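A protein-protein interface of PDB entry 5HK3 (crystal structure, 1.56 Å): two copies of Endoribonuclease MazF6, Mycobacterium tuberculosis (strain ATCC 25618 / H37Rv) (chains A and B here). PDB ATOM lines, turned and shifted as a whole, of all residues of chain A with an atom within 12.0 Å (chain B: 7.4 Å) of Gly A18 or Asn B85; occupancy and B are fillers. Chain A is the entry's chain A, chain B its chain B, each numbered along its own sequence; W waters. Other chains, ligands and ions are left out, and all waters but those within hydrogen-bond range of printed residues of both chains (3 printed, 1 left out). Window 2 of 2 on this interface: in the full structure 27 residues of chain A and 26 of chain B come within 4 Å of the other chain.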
ATOM      1  N   LEU A  13      21.173  15.545   7.881  1.00  0.00           N
ATOM      2  CA  LEU A  13      20.500  14.625   8.784  1.00  0.00           C
ATOM      3  C   LEU A  13      21.403  14.241   9.944  1.00  0.00           C
ATOM      4  O   LEU A  13      20.998  13.518  10.853  1.00  0.00           O
ATOM      5  CB  LEU A  13      20.055  13.377   8.019  1.00  0.00           C
ATOM      6  CG  LEU A  13      19.087  13.616   6.856  1.00  0.00           C
ATOM      7  CD1 LEU A  13      18.603  12.302   6.261  1.00  0.00           C
ATOM      8  CD2 LEU A  13      17.914  14.485   7.285  1.00  0.00           C
ATOM      9  N   GLY A  14      22.627  14.751   9.918  1.00  0.00           N
ATOM     10  CA  GLY A  14      23.546  14.537  11.018  1.00  0.00           C
ATOM     11  C   GLY A  14      24.581  13.481  10.710  1.00  0.00           C
ATOM     12  O   GLY A  14      24.571  12.886   9.629  1.00  0.00           O
ATOM     13  N   PRO A  15      25.488  13.240  11.666  1.00  0.00           N
ATOM     14  CA  PRO A  15      26.557  12.257  11.482  1.00  0.00           C
ATOM     15  C   PRO A  15      26.026  10.825  11.468  1.00  0.00           C
ATOM     16  O   PRO A  15      24.995  10.542  12.080  1.00  0.00           O
ATOM     17  CB  PRO A  15      27.468  12.501  12.688  1.00  0.00           C
ATOM     18  CG  PRO A  15      26.566  13.066  13.731  1.00  0.00           C
ATOM     19  CD  PRO A  15      25.540  13.881  12.992  1.00  0.00           C
ATOM     20  N   PRO A  16      26.720   9.931  10.755  1.00  0.00           N
ATOM     21  CA  PRO A  16      26.310   8.525  10.669  1.00  0.00           C
ATOM     22  C   PRO A  16      26.380   7.793  12.008  1.00  0.00           C
ATOM     23  O   PRO A  16      27.302   7.993  12.803  1.00  0.00           O
ATOM     24  CB  PRO A  16      27.302   7.924   9.659  1.00  0.00           C
ATOM     25  CG  PRO A  16      28.409   8.916   9.538  1.00  0.00           C
ATOM     26  CD  PRO A  16      27.818  10.252   9.828  1.00  0.00           C
ATOM     27  N   SER A  17      25.375   6.958  12.246  1.00  0.00           N
ATOM     28  CA  SER A  17      25.323   6.084  13.407  1.00  0.00           C
ATOM     29  C   SER A  17      24.529   4.846  13.027  1.00  0.00           C
ATOM     30  O   SER A  17      23.300   4.851  13.079  1.00  0.00           O
ATOM     31  CB  SER A  17      24.681   6.789  14.603  1.00  0.00           C
ATOM     32  OG  SER A  17      24.608   5.921  15.721  1.00  0.00           O
ATOM     33  N   GLY A  18      25.227   3.787  12.630  1.00  0.00           N
ATOM     34  CA  GLY A  18      24.553   2.601  12.139  1.00  0.00           C
ATOM     35  C   GLY A  18      23.665   2.931  10.956  1.00  0.00           C
ATOM     36  O   GLY A  18      24.085   3.624  10.026  1.00  0.00           O
ATOM     37  N   SER A  19      22.427   2.449  10.993  1.00  0.00           N
ATOM     38  CA  SER A  19      21.499   2.647   9.886  1.00  0.00           C
ATOM     39  C   SER A  19      20.550   3.820  10.111  1.00  0.00           C
ATOM     40  O   SER A  19      19.579   3.979   9.369  1.00  0.00           O
ATOM     41  CB  SER A  19      20.688   1.370   9.631  1.00  0.00           C
ATOM     42  OG  SER A  19      21.492   0.359   9.045  1.00  0.00           O
ATOM     43  N   GLN A  20      20.821   4.632  11.132  1.00  0.00           N
ATOM     44  CA  GLN A  20      20.063   5.864  11.335  1.00  0.00           C
ATOM     45  C   GLN A  20      20.182   6.745  10.106  1.00  0.00           C
ATOM     46  O   GLN A  20      21.215   6.745   9.441  1.00  0.00           O
ATOM     47  CB  GLN A  20      20.564   6.637  12.557  1.00  0.00           C
ATOM     48  CG  GLN A  20      20.186   6.053  13.897  1.00  0.00           C
ATOM     49  CD  GLN A  20      20.639   6.938  15.043  1.00  0.00           C
ATOM     50  OE1 GLN A  20      21.044   8.085  14.832  1.00  0.00           O
ATOM     51  NE2 GLN A  20      20.578   6.412  16.260  1.00  0.00           N
ATOM     52  N   PRO A  21      19.121   7.494   9.787  1.00  0.00           N
ATOM     53  CA  PRO A  21      19.247   8.485   8.714  1.00  0.00           C
ATOM     54  C   PRO A  21      20.375   9.473   9.017  1.00  0.00           C
ATOM     55  O   PRO A  21      20.520   9.911  10.157  1.00  0.00           O
ATOM     56  CB  PRO A  21      17.885   9.174   8.715  1.00  0.00           C
ATOM     57  CG  PRO A  21      16.950   8.155   9.298  1.00  0.00           C
ATOM     58  CD  PRO A  21      17.748   7.398  10.312  1.00  0.00           C
ATOM     59  N   ALA A  22      21.170   9.800   8.005  1.00  0.00           N
ATOM     60  CA  ALA A  22      22.331  10.661   8.194  1.00  0.00           C
ATOM     61  C   ALA A  22      22.762  11.313   6.881  1.00  0.00           C
ATOM     62  O   ALA A  22      22.246  10.974   5.812  1.00  0.00           O
ATOM     63  CB  ALA A  22      23.482   9.866   8.793  1.00  0.00           C
ATOM     64  N   LYS A  23      23.704  12.254   6.987  1.00  0.00           N
ATOM     65  CA  LYS A  23      24.306  12.957   5.846  1.00  0.00           C
ATOM     66  C   LYS A  23      23.331  13.928   5.179  1.00  0.00           C
ATOM     67  O   LYS A  23      22.217  14.132   5.665  1.00  0.00           O
ATOM     68  CB  LYS A  23      24.832  11.967   4.801  1.00  0.00           C
ATOM     69  CG  LYS A  23      25.816  10.924   5.325  1.00  0.00           C
ATOM     70  CD  LYS A  23      26.058   9.860   4.257  1.00  0.00           C
ATOM     71  CE  LYS A  23      27.166   8.885   4.633  1.00  0.00           C
ATOM     72  NZ  LYS A  23      27.375   7.870   3.552  1.00  0.00           N
ATOM     73  N   ARG A  25      20.741  14.763   2.493  1.00  0.00           N
ATOM     74  CA  ARG A  25      19.825  14.000   1.660  1.00  0.00           C
ATOM     75  C   ARG A  25      18.568  14.803   1.353  1.00  0.00           C
ATOM     76  O   ARG A  25      18.222  15.708   2.113  1.00  0.00           O
ATOM     77  CB  ARG A  25      19.446  12.690   2.365  1.00  0.00           C
ATOM     78  CG  ARG A  25      20.618  11.740   2.573  1.00  0.00           C
ATOM     79  CD  ARG A  25      20.175  10.416   3.156  1.00  0.00           C
ATOM     80  NE  ARG A  25      21.322   9.603   3.544  1.00  0.00           N
ATOM     81  CZ  ARG A  25      22.019   8.852   2.700  1.00  0.00           C
ATOM     82  NH1 ARG A  25      21.681   8.813   1.419  1.00  0.00           N
ATOM     83  NH2 ARG A  25      23.052   8.142   3.136  1.00  0.00           N
ATOM     84  N   VAL A  47      12.879  10.312   4.514  1.00  0.00           N
ATOM     85  CA  VAL A  47      14.115  10.420   3.745  1.00  0.00           C
ATOM     86  C   VAL A  47      13.992   9.828   2.344  1.00  0.00           C
ATOM     87  O   VAL A  47      13.429   8.749   2.163  1.00  0.00           O
ATOM     88  CB  VAL A  47      15.284   9.734   4.484  1.00  0.00           C
ATOM     89  CG1 VAL A  47      16.571   9.886   3.688  1.00  0.00           C
ATOM     90  CG2 VAL A  47      15.450  10.318   5.869  1.00  0.00           C
ATOM     91  N   THR A  49      15.977   8.600  -1.154  1.00  0.00           N
ATOM     92  CA  THR A  49      17.249   8.058  -1.641  1.00  0.00           C
ATOM     93  C   THR A  49      17.129   7.778  -3.135  1.00  0.00           C
ATOM     94  O   THR A  49      16.028   7.723  -3.661  1.00  0.00           O
ATOM     95  CB  THR A  49      17.659   6.768  -0.901  1.00  0.00           C
ATOM     96  OG1 THR A  49      16.633   5.783  -1.067  1.00  0.00           O
ATOM     97  CG2 THR A  49      17.877   7.044   0.579  1.00  0.00           C
ATOM     98  N   LEU A  54      18.723  -2.926  -1.069  1.00  0.00           N
ATOM     99  CA  LEU A  54      19.107  -3.493   0.226  1.00  0.00           C
ATOM    100  C   LEU A  54      18.308  -2.936   1.408  1.00  0.00           C
ATOM    101  O   LEU A  54      18.508  -3.357   2.549  1.00  0.00           O
ATOM    102  CB  LEU A  54      20.609  -3.298   0.483  1.00  0.00           C
ATOM    103  CG  LEU A  54      21.542  -3.925  -0.553  1.00  0.00           C
ATOM    104  CD1 LEU A  54      22.972  -3.877  -0.037  1.00  0.00           C
ATOM    105  CD2 LEU A  54      21.103  -5.343  -0.879  1.00  0.00           C
ATOM    106  N   ALA A  55      17.412  -1.985   1.141  1.00  0.00           N
ATOM    107  CA  ALA A  55      16.534  -1.430   2.172  1.00  0.00           C
ATOM    108  C   ALA A  55      15.124  -1.292   1.626  1.00  0.00           C
ATOM    109  O   ALA A  55      14.449  -0.283   1.843  1.00  0.00           O
ATOM    110  CB  ALA A  55      17.053  -0.081   2.649  1.00  0.00           C
ATOM    111  N   THR A  79      10.110   4.080   6.115  1.00  0.00           N
ATOM    112  CA  THR A  79      10.564   3.678   7.455  1.00  0.00           C
ATOM    113  C   THR A  79      11.690   4.567   7.993  1.00  0.00           C
ATOM    114  O   THR A  79      12.172   4.363   9.112  1.00  0.00           O
ATOM    115  CB  THR A  79      11.053   2.206   7.487  1.00  0.00           C
ATOM    116  OG1 THR A  79      12.220   2.060   6.665  1.00  0.00           O
ATOM    117  CG2 THR A  79       9.960   1.264   7.003  1.00  0.00           C
ATOM    118  N   ALA A  80      12.093   5.559   7.204  1.00  0.00           N
ATOM    119  CA  ALA A  80      13.166   6.477   7.577  1.00  0.00           C
ATOM    120  C   ALA A  80      12.599   7.860   7.832  1.00  0.00           C
ATOM    121  O   ALA A  80      12.490   8.683   6.925  1.00  0.00           O
ATOM    122  CB  ALA A  80      14.231   6.530   6.473  1.00  0.00           C
ATOM    123  N   ILE A  81      12.237   8.107   9.086  1.00  0.00           N
ATOM    124  CA  ILE A  81      11.564   9.338   9.461  1.00  0.00           C
ATOM    125  C   ILE A  81      12.498  10.184  10.324  1.00  0.00           C
ATOM    126  O   ILE A  81      13.179   9.672  11.218  1.00  0.00           O
ATOM    127  CB  ILE A  81      10.258   9.047  10.214  1.00  0.00           C
ATOM    128  CG1 ILE A  81       9.374   8.091   9.413  1.00  0.00           C
ATOM    129  CG2 ILE A  81       9.530  10.340  10.544  1.00  0.00           C
ATOM    130  CD1 ILE A  81       9.091   8.551   8.006  1.00  0.00           C
ATOM    131  N   VAL A  82      12.557  11.475  10.027  1.00  0.00           N
ATOM    132  CA  VAL A  82      13.410  12.394  10.758  1.00  0.00           C
ATOM    133  C   VAL A  82      12.640  13.634  11.192  1.00  0.00           C
ATOM    134  O   VAL A  82      11.629  13.997  10.597  1.00  0.00           O
ATOM    135  CB  VAL A  82      14.641  12.830   9.926  1.00  0.00           C
ATOM    136  CG1 VAL A  82      15.576  11.653   9.683  1.00  0.00           C
ATOM    137  CG2 VAL A  82      14.215  13.453   8.608  1.00  0.00           C
ATOM    138  N   ILE B   3      11.280  -6.338  19.707  1.00  0.00           N
ATOM    139  CA  ILE B   3      10.755  -5.007  19.972  1.00  0.00           C
ATOM    140  C   ILE B   3       9.308  -4.923  19.526  1.00  0.00           C
ATOM    141  O   ILE B   3       8.963  -5.386  18.444  1.00  0.00           O
ATOM    142  CB  ILE B   3      11.590  -3.926  19.250  1.00  0.00           C
ATOM    143  CG1 ILE B   3      13.014  -3.899  19.816  1.00  0.00           C
ATOM    144  CG2 ILE B   3      10.930  -2.550  19.365  1.00  0.00           C
ATOM    145  CD1 ILE B   3      14.036  -3.372  18.844  1.00  0.00           C
ATOM    146  N   ALA B  11      16.914   5.395  25.317  1.00  0.00           N
ATOM    147  CA  ALA B  11      17.701   5.451  24.094  1.00  0.00           C
ATOM    148  C   ALA B  11      18.653   6.642  24.057  1.00  0.00           C
ATOM    149  O   ALA B  11      18.345   7.722  24.571  1.00  0.00           O
ATOM    150  CB  ALA B  11      16.774   5.487  22.879  1.00  0.00           C
ATOM    151  N   LEU B  40      14.432  -5.408   8.882  1.00  0.00           N
ATOM    152  CA  LEU B  40      14.646  -3.965   8.940  1.00  0.00           C
ATOM    153  C   LEU B  40      15.491  -3.620  10.166  1.00  0.00           C
ATOM    154  O   LEU B  40      15.194  -4.076  11.272  1.00  0.00           O
ATOM    155  CB  LEU B  40      13.302  -3.234   9.006  1.00  0.00           C
ATOM    156  CG  LEU B  40      13.331  -1.707   9.119  1.00  0.00           C
ATOM    157  CD1 LEU B  40      13.972  -1.077   7.902  1.00  0.00           C
ATOM    158  CD2 LEU B  40      11.932  -1.156   9.351  1.00  0.00           C
ATOM    159  N   ALA B  41      16.536  -2.822   9.973  1.00  0.00           N
ATOM    160  CA  ALA B  41      17.507  -2.564  11.042  1.00  0.00           C
ATOM    161  C   ALA B  41      17.056  -1.519  12.046  1.00  0.00           C
ATOM    162  O   ALA B  41      17.640  -1.380  13.112  1.00  0.00           O
ATOM    163  CB  ALA B  41      18.836  -2.142  10.441  1.00  0.00           C
ATOM    164  N   THR B  42      16.020  -0.773  11.688  1.00  0.00           N
ATOM    165  CA  THR B  42      15.649   0.427  12.419  1.00  0.00           C
ATOM    166  C   THR B  42      14.236   0.360  12.964  1.00  0.00           C
ATOM    167  O   THR B  42      13.450  -0.506  12.592  1.00  0.00           O
ATOM    168  CB  THR B  42      15.764   1.674  11.527  1.00  0.00           C
ATOM    169  OG1 THR B  42      15.018   1.468  10.319  1.00  0.00           O
ATOM    170  CG2 THR B  42      17.223   1.933  11.158  1.00  0.00           C
ATOM    171  N   VAL B  43      13.945   1.273  13.887  1.00  0.00           N
ATOM    172  CA  VAL B  43      12.628   1.387  14.469  1.00  0.00           C
ATOM    173  C   VAL B  43      12.292   2.864  14.632  1.00  0.00           C
ATOM    174  O   VAL B  43      13.137   3.666  15.041  1.00  0.00           O
ATOM    175  CB  VAL B  43      12.568   0.647  15.826  1.00  0.00           C
ATOM    176  CG1 VAL B  43      13.746   1.051  16.708  1.00  0.00           C
ATOM    177  CG2 VAL B  43      11.260   0.894  16.532  1.00  0.00           C
ATOM    178  N   THR B  83      14.203   7.927  14.132  1.00  0.00           N
ATOM    179  CA  THR B  83      14.425   6.575  13.649  1.00  0.00           C
ATOM    180  C   THR B  83      15.729   6.081  14.245  1.00  0.00           C
ATOM    181  O   THR B  83      16.767   6.719  14.075  1.00  0.00           O
ATOM    182  CB  THR B  83      14.467   6.528  12.115  1.00  0.00           C
ATOM    183  OG1 THR B  83      13.225   7.025  11.607  1.00  0.00           O
ATOM    184  CG2 THR B  83      14.665   5.099  11.620  1.00  0.00           C
ATOM    185  N   LEU B  84      15.659   4.959  14.957  1.00  0.00           N
ATOM    186  CA  LEU B  84      16.785   4.452  15.746  1.00  0.00           C
ATOM    187  C   LEU B  84      17.179   3.046  15.316  1.00  0.00           C
ATOM    188  O   LEU B  84      16.386   2.320  14.747  1.00  0.00           O
ATOM    189  CB  LEU B  84      16.430   4.446  17.233  1.00  0.00           C
ATOM    190  CG  LEU B  84      16.015   5.794  17.813  1.00  0.00           C
ATOM    191  CD1 LEU B  84      15.480   5.616  19.239  1.00  0.00           C
ATOM    192  CD2 LEU B  84      17.172   6.772  17.790  1.00  0.00           C
ATOM    193  N   ASN B  85      18.420   2.658  15.576  1.00  0.00           N
ATOM    194  CA  ASN B  85      18.808   1.275  15.334  1.00  0.00           C
ATOM    195  C   ASN B  85      18.142   0.373  16.361  1.00  0.00           C
ATOM    196  O   ASN B  85      18.118   0.708  17.542  1.00  0.00           O
ATOM    197  CB  ASN B  85      20.326   1.122  15.417  1.00  0.00           C
ATOM    198  CG  ASN B  85      21.052   1.903  14.344  1.00  0.00           C
ATOM    199  OD1 ASN B  85      20.759   1.773  13.157  1.00  0.00           O
ATOM    200  ND2 ASN B  85      21.975   2.763  14.765  1.00  0.00           N
ATOM    201  N   LYS B  86      17.605  -0.766  15.927  1.00  0.00           N
ATOM    202  CA  LYS B  86      16.970  -1.701  16.859  1.00  0.00           C
ATOM    203  C   LYS B  86      17.935  -2.145  17.943  1.00  0.00           C
ATOM    204  O   LYS B  86      17.564  -2.272  19.110  1.00  0.00           O
ATOM    205  CB  LYS B  86      16.431  -2.925  16.119  1.00  0.00           C
ATOM    206  CG  LYS B  86      15.229  -2.647  15.242  1.00  0.00           C
ATOM    207  CD  LYS B  86      14.804  -3.914  14.532  1.00  0.00           C
ATOM    208  CE  LYS B  86      13.459  -3.764  13.858  1.00  0.00           C
ATOM    209  NZ  LYS B  86      13.172  -4.964  13.012  1.00  0.00           N
ATOM    210  N   THR B  87      19.190  -2.355  17.563  1.00  0.00           N
ATOM    211  CA  THR B  87      20.169  -2.871  18.515  1.00  0.00           C
ATOM    212  C   THR B  87      20.501  -1.849  19.597  1.00  0.00           C
ATOM    213  O   THR B  87      21.136  -2.186  20.597  1.00  0.00           O
ATOM    214  CB  THR B  87      21.465  -3.289  17.813  1.00  0.00           C
ATOM    215  OG1 THR B  87      21.928  -2.209  16.992  1.00  0.00           O
ATOM    216  CG2 THR B  87      21.226  -4.518  16.941  1.00  0.00           C
ATOM    217  N   ASP B  88      20.068  -0.607  19.405  1.00  0.00           N
ATOM    218  CA  ASP B  88      20.266   0.440  20.403  1.00  0.00           C
ATOM    219  C   ASP B  88      19.092   0.554  21.374  1.00  0.00           C
ATOM    220  O   ASP B  88      19.096   1.413  22.255  1.00  0.00           O
ATOM    221  CB  ASP B  88      20.502   1.785  19.723  1.00  0.00           C
ATOM    222  CG  ASP B  88      21.860   1.865  19.054  1.00  0.00           C
ATOM    223  OD1 ASP B  88      22.794   1.174  19.522  1.00  0.00           O
ATOM    224  OD2 ASP B  88      21.994   2.611  18.062  1.00  0.00           O
ATOM    225  N   LEU B  89      18.095  -0.311  21.208  1.00  0.00           N
ATOM    226  CA  LEU B  89      16.976  -0.385  22.148  1.00  0.00           C
ATOM    227  C   LEU B  89      17.098  -1.617  23.041  1.00  0.00           C
ATOM    228  O   LEU B  89      16.463  -2.640  22.787  1.00  0.00           O
ATOM    229  CB  LEU B  89      15.635  -0.420  21.422  1.00  0.00           C
ATOM    230  CG  LEU B  89      15.230   0.806  20.610  1.00  0.00           C
ATOM    231  CD1 LEU B  89      13.774   0.672  20.205  1.00  0.00           C
ATOM    232  CD2 LEU B  89      15.458   2.090  21.380  1.00  0.00           C
ATOM    233  N   THR B  90      17.938  -1.533  24.066  1.00  0.00           N
ATOM    234  CA  THR B  90      18.152  -2.669  24.954  1.00  0.00           C
ATOM    235  C   THR B  90      17.472  -2.476  26.306  1.00  0.00           C
ATOM    236  O   THR B  90      17.146  -3.443  26.996  1.00  0.00           O
ATOM    237  CB  THR B  90      19.652  -2.919  25.181  1.00  0.00           C
ATOM    238  OG1 THR B  90      19.828  -3.919  26.192  1.00  0.00           O
ATOM    239  CG2 THR B  90      20.337  -1.641  25.624  1.00  0.00           C
HETATM  240  O   HOH W   1      12.501   2.255  10.894  1.00  0.00           O
HETATM  241  O   HOH W   2      15.587  10.145  12.978  1.00  0.00           O
HETATM  242  O   HOH W   3      20.096   4.132  17.417  1.00  0.00           O
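The side-chain amide nitrogen (ND2) of Asn B85 is in hydrogen-bond range of the backbone carbonyl oxygen (O) of Ser A17 (3.0 Å).
The backbone NH (N) of Ser A19 sits at hydrogen-bond distance from the side-chain amide oxygen (OD1) of Asn B85.
The side-chain hydroxyl (OG1) of Thr B83 sits at hydrogen-bond distance from the backbone carbonyl oxygen (O) of Ile A81 (2.7 Å).
The backbone carbonyl oxygen (O) of Ala A80 sits at hydrogen-bond distance from the backbone NH (N) of Val A47, 2.9 Å away.
O of Leu B40 sits at hydrogen-bond distance from NZ of Lys B86, 2.8 Å away.
N of Lys B86 lies within hydrogen-bond range of O of Ala B41 (2.9 Å).
The backbone carbonyl oxygen of Leu B84 lies within hydrogen-bond range of the backbone NH of Val B43 (2.8 Å).
The side-chain carboxylate of Asp B88 sits at hydrogen-bond distance from the side-chain amide nitrogen of Asn B85.
Asn B85 touches Gly A18 (ND2 to CA, 3.7 Å).
Ser A19 touches Ala B41 (OG to CB, 3.9 Å).
O of Ser A19 touches CG2 of Thr B42, 3.6 Å away.
Gln A20 touches Thr B83.
Leu B84 touches Gln A20.
Gln A20 touches Asn B85 (N to OD1, 3.5 Å).
Pro A21 touches Thr B83.
Thr A79 touches Leu B40.
Thr A79 touches Thr B83 (O to CG2, 3.6 Å).
C of Ala A80 touches OG1 of Thr B83 (3.9 Å).
Leu A13 touches none of the printed residues of chain B.
Of chain B, only Asn B85 comes within 4 Å of Gly A18.
Of the printed residues of chain B, Pro A21 touches Thr B83 (3.8 Å).
Val A47 touches none of the printed residues of chain B.
Of the printed residues of chain B, Thr A79 touches Leu B40 (3.8 Å) and Thr B83 (3.6 Å).
Of the printed residues of chain B, Ile A81 touches Thr B83 (2.7 Å).
Ala B41 touches one residue of chain A.
Of chain A, only Ser A19 (3.6 Å) comes within 4 Å of Thr B42.
No residue of chain A comes within 4 Å of Val B43.
Of chain A, only Gln A20 (3.5 Å), Pro A21 (3.8 Å), Thr A79 (3.6 Å), Ala A80 (3.9 Å) and Ile A81 (2.7 Å) come within 4 Å of Thr B83.
Of chain A, only Gln A20 comes within 4 Å of Leu B84.
Of chain A, only Ser A17 (3.0 Å), Gly A18 (3.7 Å), Ser A19 (2.8 Å) and Gln A20 (3.5 Å) come within 4 Å of Asn B85.
No residue of chain A comes within 4 Å of Thr B87.
No residue of chain A comes within 4 Å of Asp B88.
The nearest residue of chain A that does not touch Asn B85 is Pro A21 (6.8 Å).
Of the 14 printed residues of chain B, 6 touch a printed residue of chain A.
Of the 20 printed residues of chain A, 8 touch a printed residue of chain B.
Printed residues of chain A that touch a printed residue of chain B: Ser A17, Gly A18, Ser A19, Gln A20, Pro A21, Thr A79, Ala A80 and Ile A81.
Hydrophobic or aromatic side chains of chain A that line the printed part of chain B: Pro A21 and Ile A81.
Among the printed residues, no Asp or Glu carboxylate lies within 4 Å of a Lys or Arg side-chain nitrogen of the other chain.
No position is printed for both chains.
Of the 13 pairs that touch across the chains among the printed residues, none has its exchanged pair printed and touching as well.
Water W3 lies within hydrogen-bond range of the side-chain carboxylate of Asp B88 (2.5 Å), the side-chain amide nitrogen of Gln A20 (2.6 Å) and the backbone NH of Asn B85 (2.9 Å).
Water W1 lies within hydrogen-bond range of the side-chain hydroxyl (OG1) of Thr B42 (2.7 Å), the backbone carbonyl oxygen (O) of Thr A79 (2.8 Å) and the backbone NH (N) of Val B43 (3.5 Å).
Water W2 lies within hydrogen-bond range of N of Thr B83 (2.9 Å) and O of Ile A81 (3.0 Å).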
